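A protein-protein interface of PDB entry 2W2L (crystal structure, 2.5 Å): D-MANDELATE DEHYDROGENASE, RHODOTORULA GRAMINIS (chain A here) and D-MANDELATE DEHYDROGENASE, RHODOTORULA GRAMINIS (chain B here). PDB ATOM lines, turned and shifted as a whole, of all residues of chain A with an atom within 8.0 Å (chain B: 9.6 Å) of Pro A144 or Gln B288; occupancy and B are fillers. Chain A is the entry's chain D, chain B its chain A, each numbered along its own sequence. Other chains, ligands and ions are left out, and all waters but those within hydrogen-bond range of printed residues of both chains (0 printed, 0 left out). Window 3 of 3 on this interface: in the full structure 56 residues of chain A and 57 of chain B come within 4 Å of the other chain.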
ATOM      1  N   ALA A 138      29.665  22.174 -23.165  1.00  0.00           N
ATOM      2  CA  ALA A 138      29.427  20.815 -22.737  1.00  0.00           C
ATOM      3  C   ALA A 138      28.064  20.685 -22.068  1.00  0.00           C
ATOM      4  O   ALA A 138      27.272  19.789 -22.437  1.00  0.00           O
ATOM      5  CB  ALA A 138      30.523  20.381 -21.799  1.00  0.00           C
ATOM      6  N   ALA A 139      27.781  21.550 -21.085  1.00  0.00           N
ATOM      7  CA  ALA A 139      26.497  21.469 -20.419  1.00  0.00           C
ATOM      8  C   ALA A 139      25.358  21.574 -21.448  1.00  0.00           C
ATOM      9  O   ALA A 139      24.410  20.825 -21.404  1.00  0.00           O
ATOM     10  CB  ALA A 139      26.355  22.515 -19.361  1.00  0.00           C
ATOM     11  N   ARG A 140      25.471  22.497 -22.389  1.00  0.00           N
ATOM     12  CA  ARG A 140      24.389  22.755 -23.325  1.00  0.00           C
ATOM     13  C   ARG A 140      24.168  21.646 -24.369  1.00  0.00           C
ATOM     14  O   ARG A 140      23.198  21.709 -25.122  1.00  0.00           O
ATOM     15  CB  ARG A 140      24.564  24.110 -24.001  1.00  0.00           C
ATOM     16  CG  ARG A 140      24.127  25.267 -23.171  1.00  0.00           C
ATOM     17  CD  ARG A 140      23.709  26.459 -24.076  1.00  0.00           C
ATOM     18  NE  ARG A 140      22.407  27.005 -23.665  1.00  0.00           N
ATOM     19  CZ  ARG A 140      22.166  27.578 -22.476  1.00  0.00           C
ATOM     20  NH1 ARG A 140      23.150  27.723 -21.599  1.00  0.00           N
ATOM     21  NH2 ARG A 140      20.951  28.027 -22.153  1.00  0.00           N
ATOM     22  N   THR A 141      25.044  20.644 -24.422  1.00  0.00           N
ATOM     23  CA  THR A 141      24.821  19.470 -25.317  1.00  0.00           C
ATOM     24  C   THR A 141      23.655  18.587 -24.831  1.00  0.00           C
ATOM     25  O   THR A 141      23.058  17.859 -25.619  1.00  0.00           O
ATOM     26  CB  THR A 141      26.060  18.552 -25.413  1.00  0.00           C
ATOM     27  OG1 THR A 141      26.342  17.990 -24.119  1.00  0.00           O
ATOM     28  CG2 THR A 141      27.293  19.317 -25.939  1.00  0.00           C
ATOM     29  N   GLY A 142      23.355  18.657 -23.529  1.00  0.00           N
ATOM     30  CA  GLY A 142      22.287  17.885 -22.928  1.00  0.00           C
ATOM     31  C   GLY A 142      22.662  16.412 -22.906  1.00  0.00           C
ATOM     32  O   GLY A 142      21.792  15.541 -22.858  1.00  0.00           O
ATOM     33  N   ASP A 143      23.960  16.132 -22.920  1.00  0.00           N
ATOM     34  CA  ASP A 143      24.456  14.779 -22.992  1.00  0.00           C
ATOM     35  C   ASP A 143      25.232  14.368 -21.711  1.00  0.00           C
ATOM     36  O   ASP A 143      26.327  14.886 -21.450  1.00  0.00           O
ATOM     37  CB  ASP A 143      25.310  14.646 -24.252  1.00  0.00           C
ATOM     38  CG  ASP A 143      25.754  13.226 -24.518  1.00  0.00           C
ATOM     39  OD1 ASP A 143      25.615  12.358 -23.627  1.00  0.00           O
ATOM     40  OD2 ASP A 143      26.270  12.980 -25.623  1.00  0.00           O
ATOM     41  N   PRO A 144      24.656  13.440 -20.915  1.00  0.00           N
ATOM     42  CA  PRO A 144      25.246  12.833 -19.727  1.00  0.00           C
ATOM     43  C   PRO A 144      26.737  12.457 -19.838  1.00  0.00           C
ATOM     44  O   PRO A 144      27.496  12.772 -18.918  1.00  0.00           O
ATOM     45  CB  PRO A 144      24.396  11.566 -19.546  1.00  0.00           C
ATOM     46  CG  PRO A 144      23.039  11.966 -20.017  1.00  0.00           C
ATOM     47  CD  PRO A 144      23.288  12.927 -21.162  1.00  0.00           C
ATOM     48  N   GLU A 145      27.156  11.794 -20.923  1.00  0.00           N
ATOM     49  CA  GLU A 145      28.567  11.386 -21.058  1.00  0.00           C
ATOM     50  C   GLU A 145      29.485  12.594 -21.219  1.00  0.00           C
ATOM     51  O   GLU A 145      30.595  12.622 -20.653  1.00  0.00           O
ATOM     52  CB  GLU A 145      28.823  10.389 -22.223  1.00  0.00           C
ATOM     53  CG  GLU A 145      28.325   8.896 -22.013  1.00  0.00           C
ATOM     54  CD  GLU A 145      28.912   8.138 -20.749  1.00  0.00           C
ATOM     55  OE1 GLU A 145      29.433   8.803 -19.802  1.00  0.00           O
ATOM     56  OE2 GLU A 145      28.836   6.873 -20.705  1.00  0.00           O
ATOM     57  N   THR A 146      29.026  13.578 -21.999  1.00  0.00           N
ATOM     58  CA  THR A 146      29.814  14.792 -22.257  1.00  0.00           C
ATOM     59  C   THR A 146      29.990  15.562 -20.945  1.00  0.00           C
ATOM     60  O   THR A 146      31.122  15.847 -20.528  1.00  0.00           O
ATOM     61  CB  THR A 146      29.218  15.662 -23.418  1.00  0.00           C
ATOM     62  OG1 THR A 146      29.025  14.827 -24.569  1.00  0.00           O
ATOM     63  CG2 THR A 146      30.155  16.831 -23.810  1.00  0.00           C
ATOM     64  N   PHE A 147      28.887  15.808 -20.257  1.00  0.00           N
ATOM     65  CA  PHE A 147      28.932  16.455 -18.942  1.00  0.00           C
ATOM     66  C   PHE A 147      30.018  15.882 -18.021  1.00  0.00           C
ATOM     67  O   PHE A 147      30.752  16.625 -17.391  1.00  0.00           O
ATOM     68  CB  PHE A 147      27.537  16.354 -18.301  1.00  0.00           C
ATOM     69  CG  PHE A 147      27.389  17.060 -16.963  1.00  0.00           C
ATOM     70  CD1 PHE A 147      26.639  18.228 -16.865  1.00  0.00           C
ATOM     71  CD2 PHE A 147      27.925  16.510 -15.792  1.00  0.00           C
ATOM     72  CE1 PHE A 147      26.462  18.872 -15.634  1.00  0.00           C
ATOM     73  CE2 PHE A 147      27.751  17.139 -14.567  1.00  0.00           C
ATOM     74  CZ  PHE A 147      27.012  18.339 -14.496  1.00  0.00           C
ATOM     75  N   ASN A 148      30.098  14.558 -17.941  1.00  0.00           N
ATOM     76  CA  ASN A 148      31.063  13.857 -17.073  1.00  0.00           C
ATOM     77  C   ASN A 148      32.505  13.901 -17.605  1.00  0.00           C
ATOM     78  O   ASN A 148      33.434  14.193 -16.846  1.00  0.00           O
ATOM     79  CB  ASN A 148      30.630  12.394 -16.849  1.00  0.00           C
ATOM     80  CG  ASN A 148      29.515  12.250 -15.822  1.00  0.00           C
ATOM     81  OD1 ASN A 148      29.364  13.063 -14.896  1.00  0.00           O
ATOM     82  ND2 ASN A 148      28.745  11.205 -15.966  1.00  0.00           N
ATOM     83  N   ARG A 149      32.691  13.605 -18.894  1.00  0.00           N
ATOM     84  CA  ARG A 149      34.027  13.658 -19.486  1.00  0.00           C
ATOM     85  C   ARG A 149      34.670  15.066 -19.308  1.00  0.00           C
ATOM     86  O   ARG A 149      35.835  15.185 -18.866  1.00  0.00           O
ATOM     87  CB  ARG A 149      34.005  13.197 -20.949  1.00  0.00           C
ATOM     88  CG  ARG A 149      35.275  13.522 -21.785  1.00  0.00           C
ATOM     89  CD  ARG A 149      35.112  13.170 -23.298  1.00  0.00           C
ATOM     90  NE  ARG A 149      33.911  13.786 -23.891  1.00  0.00           N
ATOM     91  CZ  ARG A 149      33.913  14.874 -24.671  1.00  0.00           C
ATOM     92  NH1 ARG A 149      35.058  15.476 -24.986  1.00  0.00           N
ATOM     93  NH2 ARG A 149      32.777  15.358 -25.159  1.00  0.00           N
ATOM     94  N   VAL A 150      33.888  16.107 -19.618  1.00  0.00           N
ATOM     95  CA  VAL A 150      34.310  17.499 -19.491  1.00  0.00           C
ATOM     96  C   VAL A 150      34.556  17.929 -18.004  1.00  0.00           C
ATOM     97  O   VAL A 150      35.622  18.495 -17.708  1.00  0.00           O
ATOM     98  CB  VAL A 150      33.340  18.444 -20.227  1.00  0.00           C
ATOM     99  CG1 VAL A 150      33.723  19.905 -20.034  1.00  0.00           C
ATOM    100  CG2 VAL A 150      33.285  18.102 -21.736  1.00  0.00           C
ATOM    101  N   GLY B 258      22.069  20.195  -6.880  1.00  0.00           N
ATOM    102  CA  GLY B 258      21.043  20.217  -7.934  1.00  0.00           C
ATOM    103  C   GLY B 258      19.610  20.447  -7.483  1.00  0.00           C
ATOM    104  O   GLY B 258      18.990  21.411  -7.908  1.00  0.00           O
ATOM    105  N   PRO B 259      19.072  19.554  -6.628  1.00  0.00           N
ATOM    106  CA  PRO B 259      17.684  19.569  -6.193  1.00  0.00           C
ATOM    107  C   PRO B 259      17.321  20.537  -5.044  1.00  0.00           C
ATOM    108  O   PRO B 259      16.155  20.588  -4.654  1.00  0.00           O
ATOM    109  CB  PRO B 259      17.454  18.107  -5.753  1.00  0.00           C
ATOM    110  CG  PRO B 259      18.716  17.365  -6.160  1.00  0.00           C
ATOM    111  CD  PRO B 259      19.770  18.390  -6.070  1.00  0.00           C
ATOM    112  N   GLN B 263      13.677  22.119 -10.231  1.00  0.00           N
ATOM    113  CA  GLN B 263      13.887  22.373 -11.627  1.00  0.00           C
ATOM    114  C   GLN B 263      12.597  22.862 -12.291  1.00  0.00           C
ATOM    115  O   GLN B 263      12.627  23.744 -13.132  1.00  0.00           O
ATOM    116  CB  GLN B 263      14.471  21.127 -12.282  1.00  0.00           C
ATOM    117  CG  GLN B 263      14.331  21.076 -13.782  1.00  0.00           C
ATOM    118  CD  GLN B 263      15.348  20.185 -14.430  1.00  0.00           C
ATOM    119  OE1 GLN B 263      16.532  20.176 -14.068  1.00  0.00           O
ATOM    120  NE2 GLN B 263      14.907  19.453 -15.425  1.00  0.00           N
ATOM    121  N   LEU B 280      23.115  27.951 -13.355  1.00  0.00           N
ATOM    122  CA  LEU B 280      23.144  26.688 -12.652  1.00  0.00           C
ATOM    123  C   LEU B 280      24.497  26.025 -12.903  1.00  0.00           C
ATOM    124  O   LEU B 280      24.901  25.849 -14.055  1.00  0.00           O
ATOM    125  CB  LEU B 280      21.963  25.789 -13.101  1.00  0.00           C
ATOM    126  CG  LEU B 280      20.494  26.095 -12.653  1.00  0.00           C
ATOM    127  CD1 LEU B 280      19.719  24.802 -12.475  1.00  0.00           C
ATOM    128  CD2 LEU B 280      20.352  26.878 -11.321  1.00  0.00           C
ATOM    129  N   ASP B 281      25.226  25.721 -11.837  1.00  0.00           N
ATOM    130  CA  ASP B 281      26.389  24.861 -11.934  1.00  0.00           C
ATOM    131  C   ASP B 281      25.984  23.396 -11.661  1.00  0.00           C
ATOM    132  O   ASP B 281      26.563  22.462 -12.201  1.00  0.00           O
ATOM    133  CB  ASP B 281      27.454  25.290 -10.921  1.00  0.00           C
ATOM    134  CG  ASP B 281      28.779  24.597 -11.161  1.00  0.00           C
ATOM    135  OD1 ASP B 281      29.301  24.610 -12.310  1.00  0.00           O
ATOM    136  OD2 ASP B 281      29.288  24.010 -10.206  1.00  0.00           O
ATOM    137  N   VAL B 282      24.976  23.244 -10.804  1.00  0.00           N
ATOM    138  CA  VAL B 282      24.436  21.987 -10.325  1.00  0.00           C
ATOM    139  C   VAL B 282      22.977  21.834 -10.833  1.00  0.00           C
ATOM    140  O   VAL B 282      22.238  22.816 -10.986  1.00  0.00           O
ATOM    141  CB  VAL B 282      24.538  21.932  -8.810  1.00  0.00           C
ATOM    142  CG1 VAL B 282      26.013  21.947  -8.364  1.00  0.00           C
ATOM    143  CG2 VAL B 282      23.808  23.140  -8.182  1.00  0.00           C
ATOM    144  N   HIS B 283      22.585  20.607 -11.147  1.00  0.00           N
ATOM    145  CA  HIS B 283      21.302  20.364 -11.783  1.00  0.00           C
ATOM    146  C   HIS B 283      20.523  19.250 -11.076  1.00  0.00           C
ATOM    147  O   HIS B 283      21.118  18.225 -10.683  1.00  0.00           O
ATOM    148  CB  HIS B 283      21.521  20.022 -13.242  1.00  0.00           C
ATOM    149  CG  HIS B 283      22.426  20.985 -13.947  1.00  0.00           C
ATOM    150  ND1 HIS B 283      23.790  21.011 -13.746  1.00  0.00           N
ATOM    151  CD2 HIS B 283      22.162  21.955 -14.848  1.00  0.00           C
ATOM    152  CE1 HIS B 283      24.328  21.943 -14.506  1.00  0.00           C
ATOM    153  NE2 HIS B 283      23.361  22.534 -15.181  1.00  0.00           N
ATOM    154  N   GLU B 284      19.207  19.454 -10.895  1.00  0.00           N
ATOM    155  CA  GLU B 284      18.365  18.437 -10.235  1.00  0.00           C
ATOM    156  C   GLU B 284      18.745  17.029 -10.681  1.00  0.00           C
ATOM    157  O   GLU B 284      19.083  16.199  -9.817  1.00  0.00           O
ATOM    158  CB  GLU B 284      16.848  18.642 -10.432  1.00  0.00           C
ATOM    159  CG  GLU B 284      16.033  18.211  -9.163  1.00  0.00           C
ATOM    160  CD  GLU B 284      14.499  18.217  -9.338  1.00  0.00           C
ATOM    161  OE1 GLU B 284      14.010  18.562 -10.434  1.00  0.00           O
ATOM    162  OE2 GLU B 284      13.784  17.866  -8.362  1.00  0.00           O
ATOM    163  N   PHE B 285      18.737  16.798 -11.998  1.00  0.00           N
ATOM    164  CA  PHE B 285      18.913  15.453 -12.573  1.00  0.00           C
ATOM    165  C   PHE B 285      20.334  15.195 -13.095  1.00  0.00           C
ATOM    166  O   PHE B 285      20.565  14.349 -14.000  1.00  0.00           O
ATOM    167  CB  PHE B 285      17.861  15.188 -13.683  1.00  0.00           C
ATOM    168  CG  PHE B 285      16.462  15.257 -13.185  1.00  0.00           C
ATOM    169  CD1 PHE B 285      15.739  16.447 -13.270  1.00  0.00           C
ATOM    170  CD2 PHE B 285      15.875  14.144 -12.573  1.00  0.00           C
ATOM    171  CE1 PHE B 285      14.426  16.523 -12.746  1.00  0.00           C
ATOM    172  CE2 PHE B 285      14.580  14.196 -12.060  1.00  0.00           C
ATOM    173  CZ  PHE B 285      13.847  15.390 -12.143  1.00  0.00           C
ATOM    174  N   GLU B 286      21.274  15.947 -12.520  1.00  0.00           N
ATOM    175  CA  GLU B 286      22.700  15.750 -12.738  1.00  0.00           C
ATOM    176  C   GLU B 286      23.082  14.282 -12.804  1.00  0.00           C
ATOM    177  O   GLU B 286      22.818  13.557 -11.874  1.00  0.00           O
ATOM    178  CB  GLU B 286      23.474  16.383 -11.587  1.00  0.00           C
ATOM    179  CG  GLU B 286      24.878  16.811 -11.966  1.00  0.00           C
ATOM    180  CD  GLU B 286      25.524  17.650 -10.893  1.00  0.00           C
ATOM    181  OE1 GLU B 286      26.675  17.294 -10.494  1.00  0.00           O
ATOM    182  OE2 GLU B 286      24.881  18.644 -10.445  1.00  0.00           O
ATOM    183  N   PRO B 287      23.802  13.863 -13.840  1.00  0.00           N
ATOM    184  CA  PRO B 287      24.414  14.640 -14.907  1.00  0.00           C
ATOM    185  C   PRO B 287      23.526  15.013 -16.090  1.00  0.00           C
ATOM    186  O   PRO B 287      24.023  15.560 -17.079  1.00  0.00           O
ATOM    187  CB  PRO B 287      25.565  13.731 -15.352  1.00  0.00           C
ATOM    188  CG  PRO B 287      25.046  12.373 -15.134  1.00  0.00           C
ATOM    189  CD  PRO B 287      24.158  12.433 -13.940  1.00  0.00           C
ATOM    190  N   GLN B 288      22.231  14.734 -16.029  1.00  0.00           N
ATOM    191  CA  GLN B 288      21.353  15.245 -17.096  1.00  0.00           C
ATOM    192  C   GLN B 288      20.902  16.689 -16.764  1.00  0.00           C
ATOM    193  O   GLN B 288      20.173  16.936 -15.771  1.00  0.00           O
ATOM    194  CB  GLN B 288      20.152  14.350 -17.326  1.00  0.00           C
ATOM    195  CG  GLN B 288      19.264  14.879 -18.381  1.00  0.00           C
ATOM    196  CD  GLN B 288      19.936  14.854 -19.749  1.00  0.00           C
ATOM    197  OE1 GLN B 288      20.135  13.781 -20.346  1.00  0.00           O
ATOM    198  NE2 GLN B 288      20.295  16.034 -20.253  1.00  0.00           N
ATOM    199  N   VAL B 289      21.338  17.627 -17.605  1.00  0.00           N
ATOM    200  CA  VAL B 289      20.947  19.044 -17.480  1.00  0.00           C
ATOM    201  C   VAL B 289      19.574  19.204 -18.158  1.00  0.00           C
ATOM    202  O   VAL B 289      19.345  18.633 -19.241  1.00  0.00           O
ATOM    203  CB  VAL B 289      22.024  20.005 -18.157  1.00  0.00           C
ATOM    204  CG1 VAL B 289      21.563  21.469 -18.184  1.00  0.00           C
ATOM    205  CG2 VAL B 289      23.381  19.879 -17.473  1.00  0.00           C
ATOM    206  N   SER B 290      18.677  19.983 -17.535  1.00  0.00           N
ATOM    207  CA  SER B 290      17.408  20.335 -18.181  1.00  0.00           C
ATOM    208  C   SER B 290      17.489  20.791 -19.644  1.00  0.00           C
ATOM    209  O   SER B 290      18.099  21.819 -19.993  1.00  0.00           O
ATOM    210  CB  SER B 290      16.661  21.398 -17.415  1.00  0.00           C
ATOM    211  OG  SER B 290      15.795  22.042 -18.339  1.00  0.00           O
ATOM    212  N   LYS B 291      16.800  20.052 -20.495  1.00  0.00           N
ATOM    213  CA  LYS B 291      16.763  20.391 -21.887  1.00  0.00           C
ATOM    214  C   LYS B 291      15.892  21.598 -22.198  1.00  0.00           C
ATOM    215  O   LYS B 291      16.084  22.243 -23.224  1.00  0.00           O
ATOM    216  CB  LYS B 291      16.402  19.166 -22.679  1.00  0.00           C
ATOM    217  CG  LYS B 291      17.491  18.157 -22.528  1.00  0.00           C
ATOM    218  CD  LYS B 291      17.131  16.854 -23.139  1.00  0.00           C
ATOM    219  CE  LYS B 291      17.683  16.719 -24.526  1.00  0.00           C
ATOM    220  NZ  LYS B 291      17.886  15.272 -24.772  1.00  0.00           N
ATOM    221  N   GLU B 292      14.958  21.919 -21.302  1.00  0.00           N
ATOM    222  CA  GLU B 292      14.189  23.169 -21.398  1.00  0.00           C
ATOM    223  C   GLU B 292      15.088  24.327 -21.021  1.00  0.00           C
ATOM    224  O   GLU B 292      15.261  25.237 -21.832  1.00  0.00           O
ATOM    225  CB  GLU B 292      12.947  23.178 -20.504  1.00  0.00           C
ATOM    226  CG  GLU B 292      11.794  22.273 -20.991  1.00  0.00           C
ATOM    227  CD  GLU B 292      10.890  22.910 -22.067  1.00  0.00           C
ATOM    228  OE1 GLU B 292      11.412  23.374 -23.113  1.00  0.00           O
ATOM    229  OE2 GLU B 292       9.646  22.917 -21.864  1.00  0.00           O
ATOM    230  N   LEU B 293      15.667  24.298 -19.819  1.00  0.00           N
ATOM    231  CA  LEU B 293      16.682  25.290 -19.442  1.00  0.00           C
ATOM    232  C   LEU B 293      17.676  25.579 -20.579  1.00  0.00           C
ATOM    233  O   LEU B 293      17.993  26.760 -20.812  1.00  0.00           O
ATOM    234  CB  LEU B 293      17.430  24.885 -18.197  1.00  0.00           C
ATOM    235  CG  LEU B 293      16.605  24.967 -16.917  1.00  0.00           C
ATOM    236  CD1 LEU B 293      17.530  24.865 -15.702  1.00  0.00           C
ATOM    237  CD2 LEU B 293      15.740  26.213 -16.784  1.00  0.00           C
ATOM    238  N   ILE B 294      18.110  24.536 -21.306  1.00  0.00           N
ATOM    239  CA  ILE B 294      19.104  24.671 -22.387  1.00  0.00           C
ATOM    240  C   ILE B 294      18.624  25.519 -23.523  1.00  0.00           C
ATOM    241  O   ILE B 294      19.374  26.314 -24.051  1.00  0.00           O
ATOM    242  CB  ILE B 294      19.558  23.315 -22.975  1.00  0.00           C
ATOM    243  CG1 ILE B 294      20.501  22.620 -22.020  1.00  0.00           C
ATOM    244  CG2 ILE B 294      20.236  23.502 -24.337  1.00  0.00           C
ATOM    245  CD1 ILE B 294      20.900  21.256 -22.440  1.00  0.00           C
ATOM    246  N   GLU B 295      17.378  25.330 -23.936  1.00  0.00           N
ATOM    247  CA  GLU B 295      16.828  26.096 -25.055  1.00  0.00           C
ATOM    248  C   GLU B 295      16.594  27.596 -24.735  1.00  0.00           C
ATOM    249  O   GLU B 295      16.603  28.428 -25.633  1.00  0.00           O
ATOM    250  CB  GLU B 295      15.590  25.396 -25.596  1.00  0.00           C
ATOM    251  CG  GLU B 295      15.882  24.429 -26.808  1.00  0.00           C
ATOM    252  CD  GLU B 295      17.004  23.326 -26.604  1.00  0.00           C
ATOM    253  OE1 GLU B 295      17.135  22.683 -25.512  1.00  0.00           O
ATOM    254  OE2 GLU B 295      17.748  23.070 -27.585  1.00  0.00           O
ATOM    255  N   LEU B 301      24.490  27.621 -17.962  1.00  0.00           N
ATOM    256  CA  LEU B 301      24.686  26.268 -17.405  1.00  0.00           C
ATOM    257  C   LEU B 301      26.110  25.714 -17.444  1.00  0.00           C
ATOM    258  O   LEU B 301      26.720  25.703 -18.504  1.00  0.00           O
ATOM    259  CB  LEU B 301      23.725  25.289 -18.084  1.00  0.00           C
ATOM    260  CG  LEU B 301      22.254  25.700 -18.069  1.00  0.00           C
ATOM    261  CD1 LEU B 301      21.670  24.854 -19.108  1.00  0.00           C
ATOM    262  CD2 LEU B 301      21.572  25.487 -16.720  1.00  0.00           C
ATOM    263  N   THR B 302      26.628  25.254 -16.301  1.00  0.00           N
ATOM    264  CA  THR B 302      27.935  24.612 -16.318  1.00  0.00           C
ATOM    265  C   THR B 302      27.958  23.208 -15.717  1.00  0.00           C
ATOM    266  O   THR B 302      27.098  22.891 -14.882  1.00  0.00           O
ATOM    267  CB  THR B 302      29.000  25.401 -15.565  1.00  0.00           C
ATOM    268  OG1 THR B 302      28.544  25.582 -14.239  1.00  0.00           O
ATOM    269  CG2 THR B 302      29.300  26.735 -16.242  1.00  0.00           C
ATOM    270  N   THR B 303      28.991  22.415 -16.084  1.00  0.00           N
ATOM    271  CA  THR B 303      29.140  21.011 -15.677  1.00  0.00           C
ATOM    272  C   THR B 303      29.734  20.866 -14.278  1.00  0.00           C
ATOM    273  O   THR B 303      30.806  20.281 -14.078  1.00  0.00           O
ATOM    274  CB  THR B 303      29.914  20.148 -16.702  1.00  0.00           C
ATOM    275  OG1 THR B 303      31.248  20.639 -16.826  1.00  0.00           O
ATOM    276  CG2 THR B 303      29.298  20.218 -18.097  1.00  0.00           C
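Hydrophobic or aromatic side chains of chain B within 4 Å of the printed part of chain A: His B283, Pro B287, Val B289 and Ile B294.
Hydrophobic or aromatic side chains of chain A that line the printed part of chain B: Ala A138, Ala A139, Pro A144 and Phe A147.
Among the printed residues, 17 pairs touch across the chains.
The backbone carbonyl oxygen (O) of Asp B281 lies close to a ring nitrogen (ND1) of His B283, at 3.5 Å.
The backbone NH (N) of His B283 lies within hydrogen-bond range of the side-chain carboxylate (OE2) of Glu B286, 3.1 Å away.
N of Leu B293 lies within hydrogen-bond range of OG of Ser B290.
The side-chain hydroxyl (OG1) of Thr A141 sits at hydrogen-bond distance from the backbone carbonyl oxygen (O) of Ala A138, 2.6 Å away.
Gln B288 touches two residues of chain A.
Of chain B, only Gln B288 (3.0 Å) and Ile B294 (3.7 Å) come within 4 Å of Gly A142.
Printed residues of chain B within 4 Å of Ala A139: Ile B294 (3.7 Å), Leu B301 (3.3 Å) and Thr B303 (3.6 Å).
Of the printed residues of chain B, Phe A147 touches His B283 (3.9 Å), Glu B286 (3.6 Å), Pro B287 (3.7 Å), Val B289 (3.7 Å) and Thr B303 (3.4 Å).
Glu B284 touches none of the printed residues of chain A.
Gly B258 touches none of the printed residues of chain A.
The nearest printed residue of chain A that does not touch Val B289 is Ala A139 (4.1 Å).
Among the printed residues, pairs that only touch across the chains: Ala A138 with Thr B303 (3.9 Å), Ala A139 with Ile B294 (3.7 Å), Ala A139 with Leu B301 (3.3 Å), Ala A139 with Thr B303 (3.6 Å), Arg A140 with Leu B301 (3.9 Å), Gly A142 with Ile B294 (3.7 Å), Pro A144 with Pro B287 (3.99 Å), Pro A144 with Gln B288 (3.4 Å), Phe A147 with His B283 (3.9 Å), Phe A147 with Glu B286 (3.6 Å), Phe A147 with Pro B287 (3.7 Å), Phe A147 with Val B289 (3.7 Å), Phe A147 with Thr B303 (3.4 Å) and Asn A148 with Pro B287 (3.9 Å).
The backbone carbonyl oxygen (O) of Gly A142 is in hydrogen-bond range of the side-chain amide nitrogen (NE2) of Gln B288, at 3.0 Å.
O of Leu B293 is in hydrogen-bond range of NH2 of Arg A140, 3.5 Å away.
O of Ile B294 sits at hydrogen-bond distance from NH2 of Arg A140, at 3.0 Å.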
